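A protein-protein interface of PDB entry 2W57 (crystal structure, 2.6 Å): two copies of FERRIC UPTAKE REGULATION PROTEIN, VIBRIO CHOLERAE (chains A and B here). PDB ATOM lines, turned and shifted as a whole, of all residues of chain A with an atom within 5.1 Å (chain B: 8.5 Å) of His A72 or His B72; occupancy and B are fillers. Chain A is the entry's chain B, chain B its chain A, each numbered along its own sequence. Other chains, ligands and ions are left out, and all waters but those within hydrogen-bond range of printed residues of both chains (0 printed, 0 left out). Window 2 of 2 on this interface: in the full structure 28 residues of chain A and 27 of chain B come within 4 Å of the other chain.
The backbone NH of Ser B126 sits at hydrogen-bond distance from the backbone carbonyl oxygen of Tyr A128 (2.8 Å).
ND1 of His A71 sits at hydrogen-bond distance from OH of Tyr A128 (2.6 Å).
The side-chain hydroxyl of Tyr A130 sits close to the backbone NH of Glu A74 (3.5 Å).
His A72 touches His B72.
Tyr A130 touches Ser B126.
Of chain B, only His B72 (3.5 Å) comes within 4 Å of His A72.
His B72 touches just one residue of chain A: His A72 (3.5 Å).
Printed residues of chain B within 4 Å of Tyr A130: Ser B126 (3.6 Å).
Printed residues of chain A within 4 Å of Ser B126: Tyr A128 and Tyr A130.
Of the printed residues of chain B, Tyr A128 touches Ser B126 (2.8 Å).
His B71 touches none of the printed residues of chain A.
His B90 touches none of the printed residues of chain A.
The nearest residue of chain B that does not touch His A72 is Phe B73 (5.1 Å).
Of the 18 printed residues of chain B, 2 touch a printed residue of chain A.
Printed residues of chain B that touch a printed residue of chain A: His B72 and Ser B126.
Hydrophobic or aromatic side chains of chain B that line the printed part of chain A: His B72.
Among the printed residues, no Asp or Glu carboxylate lies within 4 Å of a Lys or Arg side-chain nitrogen of the other chain.
His B72 touches its own counterpart, His A72.
Positions printed for both chains: 70, 71, 72, 73, 74, 77, 78, 128 and 130.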
ATOM      1  N   ARG A  70      30.340 -13.606 -25.826  1.00  0.00           N
ATOM      2  CA  ARG A  70      31.205 -14.775 -25.679  1.00  0.00           C
ATOM      3  C   ARG A  70      30.679 -15.929 -26.510  1.00  0.00           C
ATOM      4  O   ARG A  70      29.483 -16.195 -26.486  1.00  0.00           O
ATOM      5  CB  ARG A  70      31.219 -15.214 -24.222  1.00  0.00           C
ATOM      6  CG  ARG A  70      32.380 -16.098 -23.898  1.00  0.00           C
ATOM      7  CD  ARG A  70      32.157 -16.812 -22.601  1.00  0.00           C
ATOM      8  NE  ARG A  70      32.210 -15.910 -21.464  1.00  0.00           N
ATOM      9  CZ  ARG A  70      33.161 -15.946 -20.538  1.00  0.00           C
ATOM     10  NH1 ARG A  70      34.132 -16.858 -20.626  1.00  0.00           N
ATOM     11  NH2 ARG A  70      33.139 -15.077 -19.522  1.00  0.00           N
ATOM     12  N   HIS A  71      31.549 -16.623 -27.236  1.00  0.00           N
ATOM     13  CA  HIS A  71      31.128 -17.801 -27.991  1.00  0.00           C
ATOM     14  C   HIS A  71      31.880 -18.996 -27.477  1.00  0.00           C
ATOM     15  O   HIS A  71      33.112 -19.005 -27.497  1.00  0.00           O
ATOM     16  CB  HIS A  71      31.420 -17.668 -29.486  1.00  0.00           C
ATOM     17  CG  HIS A  71      30.908 -16.405 -30.100  1.00  0.00           C
ATOM     18  ND1 HIS A  71      29.566 -16.180 -30.337  1.00  0.00           N
ATOM     19  CD2 HIS A  71      31.559 -15.297 -30.526  1.00  0.00           C
ATOM     20  CE1 HIS A  71      29.415 -14.983 -30.876  1.00  0.00           C
ATOM     21  NE2 HIS A  71      30.610 -14.428 -30.998  1.00  0.00           N
ATOM     22  N   HIS A  72      31.145 -20.006 -27.019  1.00  0.00           N
ATOM     23  CA  HIS A  72      31.763 -21.248 -26.587  1.00  0.00           C
ATOM     24  C   HIS A  72      31.856 -22.126 -27.805  1.00  0.00           C
ATOM     25  O   HIS A  72      30.841 -22.445 -28.424  1.00  0.00           O
ATOM     26  CB  HIS A  72      30.955 -21.917 -25.479  1.00  0.00           C
ATOM     27  CG  HIS A  72      30.778 -21.063 -24.263  1.00  0.00           C
ATOM     28  ND1 HIS A  72      31.615 -21.143 -23.171  1.00  0.00           N
ATOM     29  CD2 HIS A  72      29.865 -20.103 -23.972  1.00  0.00           C
ATOM     30  CE1 HIS A  72      31.220 -20.276 -22.254  1.00  0.00           C
ATOM     31  NE2 HIS A  72      30.163 -19.631 -22.716  1.00  0.00           N
ATOM     32  N   PHE A  73      33.092 -22.473 -28.163  1.00  0.00           N
ATOM     33  CA  PHE A  73      33.378 -23.275 -29.349  1.00  0.00           C
ATOM     34  C   PHE A  73      33.772 -24.703 -28.961  1.00  0.00           C
ATOM     35  O   PHE A  73      34.166 -24.959 -27.813  1.00  0.00           O
ATOM     36  CB  PHE A  73      34.480 -22.624 -30.212  1.00  0.00           C
ATOM     37  CG  PHE A  73      34.032 -21.409 -31.001  1.00  0.00           C
ATOM     38  CD1 PHE A  73      32.686 -21.177 -31.287  1.00  0.00           C
ATOM     39  CD2 PHE A  73      34.975 -20.516 -31.504  1.00  0.00           C
ATOM     40  CE1 PHE A  73      32.281 -20.046 -32.040  1.00  0.00           C
ATOM     41  CE2 PHE A  73      34.589 -19.381 -32.249  1.00  0.00           C
ATOM     42  CZ  PHE A  73      33.241 -19.150 -32.514  1.00  0.00           C
ATOM     43  N   GLU A  74      33.664 -25.616 -29.934  1.00  0.00           N
ATOM     44  CA  GLU A  74      33.903 -27.062 -29.751  1.00  0.00           C
ATOM     45  C   GLU A  74      35.238 -27.311 -29.052  1.00  0.00           C
ATOM     46  O   GLU A  74      36.289 -26.838 -29.517  1.00  0.00           O
ATOM     47  CB  GLU A  74      33.874 -27.779 -31.109  1.00  0.00           C
ATOM     48  CG  GLU A  74      33.759 -29.322 -31.041  1.00  0.00           C
ATOM     49  CD  GLU A  74      34.006 -30.008 -32.393  1.00  0.00           C
ATOM     50  OE1 GLU A  74      34.458 -29.328 -33.340  1.00  0.00           O
ATOM     51  OE2 GLU A  74      33.758 -31.230 -32.515  1.00  0.00           O
ATOM     52  N   LYS A  77      36.616 -23.777 -25.546  1.00  0.00           N
ATOM     53  CA  LYS A  77      37.289 -22.475 -25.608  1.00  0.00           C
ATOM     54  C   LYS A  77      36.287 -21.346 -25.854  1.00  0.00           C
ATOM     55  O   LYS A  77      35.273 -21.538 -26.545  1.00  0.00           O
ATOM     56  CB  LYS A  77      38.372 -22.448 -26.692  1.00  0.00           C
ATOM     57  CG  LYS A  77      39.440 -21.371 -26.452  1.00  0.00           C
ATOM     58  CD  LYS A  77      39.827 -20.671 -27.758  1.00  0.00           C
ATOM     59  CE  LYS A  77      40.773 -21.526 -28.617  1.00  0.00           C
ATOM     60  NZ  LYS A  77      40.790 -21.077 -30.044  1.00  0.00           N
ATOM     61  N   SER A  78      36.588 -20.179 -25.278  1.00  0.00           N
ATOM     62  CA  SER A  78      35.782 -18.973 -25.436  1.00  0.00           C
ATOM     63  C   SER A  78      36.449 -17.994 -26.414  1.00  0.00           C
ATOM     64  O   SER A  78      37.620 -17.644 -26.253  1.00  0.00           O
ATOM     65  CB  SER A  78      35.548 -18.295 -24.075  1.00  0.00           C
ATOM     66  OG  SER A  78      34.659 -19.041 -23.251  1.00  0.00           O
ATOM     67  N   TYR A 128      27.231 -21.950 -35.172  1.00  0.00           N
ATOM     68  CA  TYR A 128      28.650 -22.238 -35.288  1.00  0.00           C
ATOM     69  C   TYR A 128      28.847 -23.521 -36.069  1.00  0.00           C
ATOM     70  O   TYR A 128      28.389 -24.586 -35.663  1.00  0.00           O
ATOM     71  CB  TYR A 128      29.332 -22.353 -33.919  1.00  0.00           C
ATOM     72  CG  TYR A 128      28.988 -21.278 -32.896  1.00  0.00           C
ATOM     73  CD1 TYR A 128      28.719 -19.961 -33.281  1.00  0.00           C
ATOM     74  CD2 TYR A 128      28.977 -21.581 -31.526  1.00  0.00           C
ATOM     75  CE1 TYR A 128      28.421 -18.987 -32.344  1.00  0.00           C
ATOM     76  CE2 TYR A 128      28.697 -20.608 -30.575  1.00  0.00           C
ATOM     77  CZ  TYR A 128      28.414 -19.315 -30.991  1.00  0.00           C
ATOM     78  OH  TYR A 128      28.126 -18.348 -30.052  1.00  0.00           O
ATOM     79  N   TYR A 130      31.675 -26.023 -37.367  1.00  0.00           N
ATOM     80  CA  TYR A 130      33.053 -26.394 -37.067  1.00  0.00           C
ATOM     81  C   TYR A 130      33.601 -27.260 -38.178  1.00  0.00           C
ATOM     82  O   TYR A 130      32.860 -28.052 -38.771  1.00  0.00           O
ATOM     83  CB  TYR A 130      33.124 -27.151 -35.744  1.00  0.00           C
ATOM     84  CG  TYR A 130      32.504 -26.408 -34.596  1.00  0.00           C
ATOM     85  CD1 TYR A 130      33.136 -25.290 -34.044  1.00  0.00           C
ATOM     86  CD2 TYR A 130      31.280 -26.812 -34.057  1.00  0.00           C
ATOM     87  CE1 TYR A 130      32.562 -24.588 -32.986  1.00  0.00           C
ATOM     88  CE2 TYR A 130      30.702 -26.116 -32.988  1.00  0.00           C
ATOM     89  CZ  TYR A 130      31.356 -25.010 -32.467  1.00  0.00           C
ATOM     90  OH  TYR A 130      30.805 -24.321 -31.426  1.00  0.00           O
ATOM     91  N   ASP B  63      29.644 -35.572 -18.001  1.00  0.00           N
ATOM     92  CA  ASP B  63      30.061 -34.977 -19.277  1.00  0.00           C
ATOM     93  C   ASP B  63      31.265 -35.737 -19.877  1.00  0.00           C
ATOM     94  O   ASP B  63      31.206 -36.213 -21.011  1.00  0.00           O
ATOM     95  CB  ASP B  63      30.371 -33.492 -19.104  1.00  0.00           C
ATOM     96  CG  ASP B  63      30.417 -32.743 -20.424  1.00  0.00           C
ATOM     97  OD1 ASP B  63      30.483 -33.383 -21.494  1.00  0.00           O
ATOM     98  OD2 ASP B  63      30.385 -31.500 -20.397  1.00  0.00           O
ATOM     99  N   THR B  69      25.580 -34.474 -22.289  1.00  0.00           N
ATOM    100  CA  THR B  69      26.164 -33.472 -23.169  1.00  0.00           C
ATOM    101  C   THR B  69      25.897 -32.112 -22.551  1.00  0.00           C
ATOM    102  O   THR B  69      24.760 -31.829 -22.144  1.00  0.00           O
ATOM    103  CB  THR B  69      25.499 -33.493 -24.561  1.00  0.00           C
ATOM    104  OG1 THR B  69      25.667 -34.787 -25.164  1.00  0.00           O
ATOM    105  CG2 THR B  69      26.113 -32.429 -25.475  1.00  0.00           C
ATOM    106  N   ARG B  70      26.934 -31.274 -22.475  1.00  0.00           N
ATOM    107  CA  ARG B  70      26.774 -29.898 -22.006  1.00  0.00           C
ATOM    108  C   ARG B  70      26.561 -28.936 -23.163  1.00  0.00           C
ATOM    109  O   ARG B  70      27.333 -28.929 -24.117  1.00  0.00           O
ATOM    110  CB  ARG B  70      27.968 -29.423 -21.162  1.00  0.00           C
ATOM    111  CG  ARG B  70      27.600 -28.225 -20.275  1.00  0.00           C
ATOM    112  CD  ARG B  70      28.767 -27.301 -19.906  1.00  0.00           C
ATOM    113  NE  ARG B  70      29.565 -27.802 -18.788  1.00  0.00           N
ATOM    114  CZ  ARG B  70      29.709 -27.203 -17.600  1.00  0.00           C
ATOM    115  NH1 ARG B  70      29.108 -26.043 -17.309  1.00  0.00           N
ATOM    116  NH2 ARG B  70      30.481 -27.780 -16.689  1.00  0.00           N
ATOM    117  N   HIS B  71      25.517 -28.119 -23.053  1.00  0.00           N
ATOM    118  CA  HIS B  71      25.296 -27.005 -23.972  1.00  0.00           C
ATOM    119  C   HIS B  71      25.447 -25.676 -23.250  1.00  0.00           C
ATOM    120  O   HIS B  71      24.888 -25.495 -22.166  1.00  0.00           O
ATOM    121  CB  HIS B  71      23.890 -27.068 -24.567  1.00  0.00           C
ATOM    122  CG  HIS B  71      23.627 -28.293 -25.381  1.00  0.00           C
ATOM    123  ND1 HIS B  71      24.040 -28.420 -26.692  1.00  0.00           N
ATOM    124  CD2 HIS B  71      22.985 -29.445 -25.075  1.00  0.00           C
ATOM    125  CE1 HIS B  71      23.672 -29.601 -27.154  1.00  0.00           C
ATOM    126  NE2 HIS B  71      23.026 -30.240 -26.193  1.00  0.00           N
ATOM    127  N   HIS B  72      26.176 -24.738 -23.855  1.00  0.00           N
ATOM    128  CA  HIS B  72      26.309 -23.390 -23.291  1.00  0.00           C
ATOM    129  C   HIS B  72      25.340 -22.428 -23.966  1.00  0.00           C
ATOM    130  O   HIS B  72      25.527 -22.072 -25.128  1.00  0.00           O
ATOM    131  CB  HIS B  72      27.725 -22.886 -23.469  1.00  0.00           C
ATOM    132  CG  HIS B  72      28.752 -23.706 -22.761  1.00  0.00           C
ATOM    133  ND1 HIS B  72      29.242 -23.371 -21.514  1.00  0.00           N
ATOM    134  CD2 HIS B  72      29.403 -24.835 -23.132  1.00  0.00           C
ATOM    135  CE1 HIS B  72      30.143 -24.265 -21.146  1.00  0.00           C
ATOM    136  NE2 HIS B  72      30.257 -25.165 -22.107  1.00  0.00           N
ATOM    137  N   PHE B  73      24.300 -22.009 -23.251  1.00  0.00           N
ATOM    138  CA  PHE B  73      23.264 -21.151 -23.838  1.00  0.00           C
ATOM    139  C   PHE B  73      23.681 -19.695 -23.861  1.00  0.00           C
ATOM    140  O   PHE B  73      24.817 -19.367 -23.509  1.00  0.00           O
ATOM    141  CB  PHE B  73      21.950 -21.308 -23.083  1.00  0.00           C
ATOM    142  CG  PHE B  73      21.109 -22.436 -23.576  1.00  0.00           C
ATOM    143  CD1 PHE B  73      21.609 -23.342 -24.512  1.00  0.00           C
ATOM    144  CD2 PHE B  73      19.817 -22.617 -23.085  1.00  0.00           C
ATOM    145  CE1 PHE B  73      20.831 -24.396 -24.969  1.00  0.00           C
ATOM    146  CE2 PHE B  73      19.029 -23.679 -23.531  1.00  0.00           C
ATOM    147  CZ  PHE B  73      19.536 -24.568 -24.478  1.00  0.00           C
ATOM    148  N   GLU B  74      22.754 -18.827 -24.266  1.00  0.00           N
ATOM    149  CA  GLU B  74      23.031 -17.400 -24.417  1.00  0.00           C
ATOM    150  C   GLU B  74      23.476 -16.793 -23.099  1.00  0.00           C
ATOM    151  O   GLU B  74      22.745 -16.811 -22.097  1.00  0.00           O
ATOM    152  CB  GLU B  74      21.816 -16.639 -24.965  1.00  0.00           C
ATOM    153  CG  GLU B  74      22.168 -15.281 -25.614  1.00  0.00           C
ATOM    154  CD  GLU B  74      20.926 -14.458 -25.996  1.00  0.00           C
ATOM    155  OE1 GLU B  74      19.797 -15.038 -26.038  1.00  0.00           O
ATOM    156  OE2 GLU B  74      21.087 -13.226 -26.247  1.00  0.00           O
ATOM    157  N   GLY B  75      24.703 -16.284 -23.127  1.00  0.00           N
ATOM    158  CA  GLY B  75      25.344 -15.658 -21.974  1.00  0.00           C
ATOM    159  C   GLY B  75      25.056 -16.240 -20.595  1.00  0.00           C
ATOM    160  O   GLY B  75      24.255 -15.684 -19.850  1.00  0.00           O
ATOM    161  N   GLY B  76      25.709 -17.348 -20.257  1.00  0.00           N
ATOM    162  CA  GLY B  76      25.736 -17.818 -18.879  1.00  0.00           C
ATOM    163  C   GLY B  76      25.324 -19.258 -18.691  1.00  0.00           C
ATOM    164  O   GLY B  76      26.139 -20.092 -18.317  1.00  0.00           O
ATOM    165  N   LYS B  77      24.058 -19.545 -18.967  1.00  0.00           N
ATOM    166  CA  LYS B  77      23.453 -20.845 -18.698  1.00  0.00           C
ATOM    167  C   LYS B  77      24.100 -22.030 -19.443  1.00  0.00           C
ATOM    168  O   LYS B  77      24.193 -22.023 -20.671  1.00  0.00           O
ATOM    169  CB  LYS B  77      21.969 -20.767 -19.042  1.00  0.00           C
ATOM    170  CG  LYS B  77      21.085 -21.817 -18.402  1.00  0.00           C
ATOM    171  CD  LYS B  77      19.643 -21.516 -18.767  1.00  0.00           C
ATOM    172  CE  LYS B  77      18.676 -22.168 -17.815  1.00  0.00           C
ATOM    173  NZ  LYS B  77      17.281 -21.796 -18.183  1.00  0.00           N
ATOM    174  N   SER B  78      24.552 -23.027 -18.677  1.00  0.00           N
ATOM    175  CA  SER B  78      24.837 -24.366 -19.191  1.00  0.00           C
ATOM    176  C   SER B  78      23.644 -25.247 -18.899  1.00  0.00           C
ATOM    177  O   SER B  78      23.177 -25.305 -17.764  1.00  0.00           O
ATOM    178  CB  SER B  78      26.040 -24.997 -18.495  1.00  0.00           C
ATOM    179  OG  SER B  78      27.185 -24.177 -18.558  1.00  0.00           O
ATOM    180  N   VAL B  79      23.148 -25.934 -19.920  1.00  0.00           N
ATOM    181  CA  VAL B  79      22.119 -26.952 -19.735  1.00  0.00           C
ATOM    182  C   VAL B  79      22.662 -28.308 -20.166  1.00  0.00           C
ATOM    183  O   VAL B  79      23.513 -28.415 -21.068  1.00  0.00           O
ATOM    184  CB  VAL B  79      20.779 -26.622 -20.473  1.00  0.00           C
ATOM    185  CG1 VAL B  79      20.135 -25.365 -19.902  1.00  0.00           C
ATOM    186  CG2 VAL B  79      20.991 -26.454 -21.955  1.00  0.00           C
ATOM    187  N   PHE B  80      22.162 -29.343 -19.512  1.00  0.00           N
ATOM    188  CA  PHE B  80      22.615 -30.690 -19.735  1.00  0.00           C
ATOM    189  C   PHE B  80      21.446 -31.546 -20.213  1.00  0.00           C
ATOM    190  O   PHE B  80      20.282 -31.209 -20.005  1.00  0.00           O
ATOM    191  CB  PHE B  80      23.203 -31.257 -18.443  1.00  0.00           C
ATOM    192  CG  PHE B  80      24.382 -30.469 -17.897  1.00  0.00           C
ATOM    193  CD1 PHE B  80      25.684 -30.923 -18.085  1.00  0.00           C
ATOM    194  CD2 PHE B  80      24.183 -29.286 -17.174  1.00  0.00           C
ATOM    195  CE1 PHE B  80      26.771 -30.220 -17.572  1.00  0.00           C
ATOM    196  CE2 PHE B  80      25.262 -28.566 -16.664  1.00  0.00           C
ATOM    197  CZ  PHE B  80      26.564 -29.032 -16.865  1.00  0.00           C
ATOM    198  N   HIS B  90      18.392 -26.616 -31.206  1.00  0.00           N
ATOM    199  CA  HIS B  90      17.589 -26.140 -30.091  1.00  0.00           C
ATOM    200  C   HIS B  90      16.964 -24.796 -30.326  1.00  0.00           C
ATOM    201  O   HIS B  90      17.594 -23.869 -30.812  1.00  0.00           O
ATOM    202  CB  HIS B  90      18.404 -26.127 -28.792  1.00  0.00           C
ATOM    203  CG  HIS B  90      19.143 -27.403 -28.526  1.00  0.00           C
ATOM    204  ND1 HIS B  90      20.340 -27.713 -29.143  1.00  0.00           N
ATOM    205  CD2 HIS B  90      18.858 -28.448 -27.712  1.00  0.00           C
ATOM    206  CE1 HIS B  90      20.755 -28.896 -28.723  1.00  0.00           C
ATOM    207  NE2 HIS B  90      19.877 -29.361 -27.850  1.00  0.00           N
ATOM    208  N   VAL B  92      14.999 -22.038 -28.034  1.00  0.00           N
ATOM    209  CA  VAL B  92      14.940 -21.772 -26.610  1.00  0.00           C
ATOM    210  C   VAL B  92      14.030 -20.581 -26.345  1.00  0.00           C
ATOM    211  O   VAL B  92      14.191 -19.523 -26.971  1.00  0.00           O
ATOM    212  CB  VAL B  92      16.356 -21.505 -26.074  1.00  0.00           C
ATOM    213  CG1 VAL B  92      16.355 -21.256 -24.579  1.00  0.00           C
ATOM    214  CG2 VAL B  92      17.268 -22.666 -26.428  1.00  0.00           C
ATOM    215  N   SER B 126      26.761 -26.350 -34.167  1.00  0.00           N
ATOM    216  CA  SER B 126      25.762 -26.165 -33.118  1.00  0.00           C
ATOM    217  C   SER B 126      24.885 -24.984 -33.468  1.00  0.00           C
ATOM    218  O   SER B 126      25.384 -23.959 -33.931  1.00  0.00           O
ATOM    219  CB  SER B 126      26.410 -25.994 -31.731  1.00  0.00           C
ATOM    220  OG  SER B 126      27.268 -24.868 -31.683  1.00  0.00           O
ATOM    221  N   TYR B 128      21.501 -22.619 -32.066  1.00  0.00           N
ATOM    222  CA  TYR B 128      20.610 -22.222 -30.977  1.00  0.00           C
ATOM    223  C   TYR B 128      19.754 -21.048 -31.412  1.00  0.00           C
ATOM    224  O   TYR B 128      20.273 -19.994 -31.771  1.00  0.00           O
ATOM    225  CB  TYR B 128      21.405 -21.840 -29.718  1.00  0.00           C
ATOM    226  CG  TYR B 128      22.233 -22.967 -29.169  1.00  0.00           C
ATOM    227  CD1 TYR B 128      21.650 -23.987 -28.428  1.00  0.00           C
ATOM    228  CD2 TYR B 128      23.598 -23.036 -29.419  1.00  0.00           C
ATOM    229  CE1 TYR B 128      22.412 -25.050 -27.946  1.00  0.00           C
ATOM    230  CE2 TYR B 128      24.369 -24.090 -28.943  1.00  0.00           C
ATOM    231  CZ  TYR B 128      23.773 -25.091 -28.210  1.00  0.00           C
ATOM    232  OH  TYR B 128      24.537 -26.137 -27.731  1.00  0.00           O
ATOM    233  N   TYR B 130      16.930 -18.390 -30.140  1.00  0.00           N
ATOM    234  CA  TYR B 130      16.328 -17.876 -28.911  1.00  0.00           C
ATOM    235  C   TYR B 130      15.150 -16.957 -29.231  1.00  0.00           C
ATOM    236  O   TYR B 130      15.229 -16.154 -30.156  1.00  0.00           O
ATOM    237  CB  TYR B 130      17.364 -17.145 -28.055  1.00  0.00           C
ATOM    238  CG  TYR B 130      18.639 -17.921 -27.767  1.00  0.00           C
ATOM    239  CD1 TYR B 130      18.746 -18.719 -26.630  1.00  0.00           C
ATOM    240  CD2 TYR B 130      19.752 -17.830 -28.611  1.00  0.00           C
ATOM    241  CE1 TYR B 130      19.909 -19.415 -26.339  1.00  0.00           C
ATOM    242  CE2 TYR B 130      20.923 -18.526 -28.329  1.00  0.00           C
ATOM    243  CZ  TYR B 130      20.991 -19.317 -27.185  1.00  0.00           C
ATOM    244  OH  TYR B 130      22.134 -20.024 -26.882  1.00  0.00           O
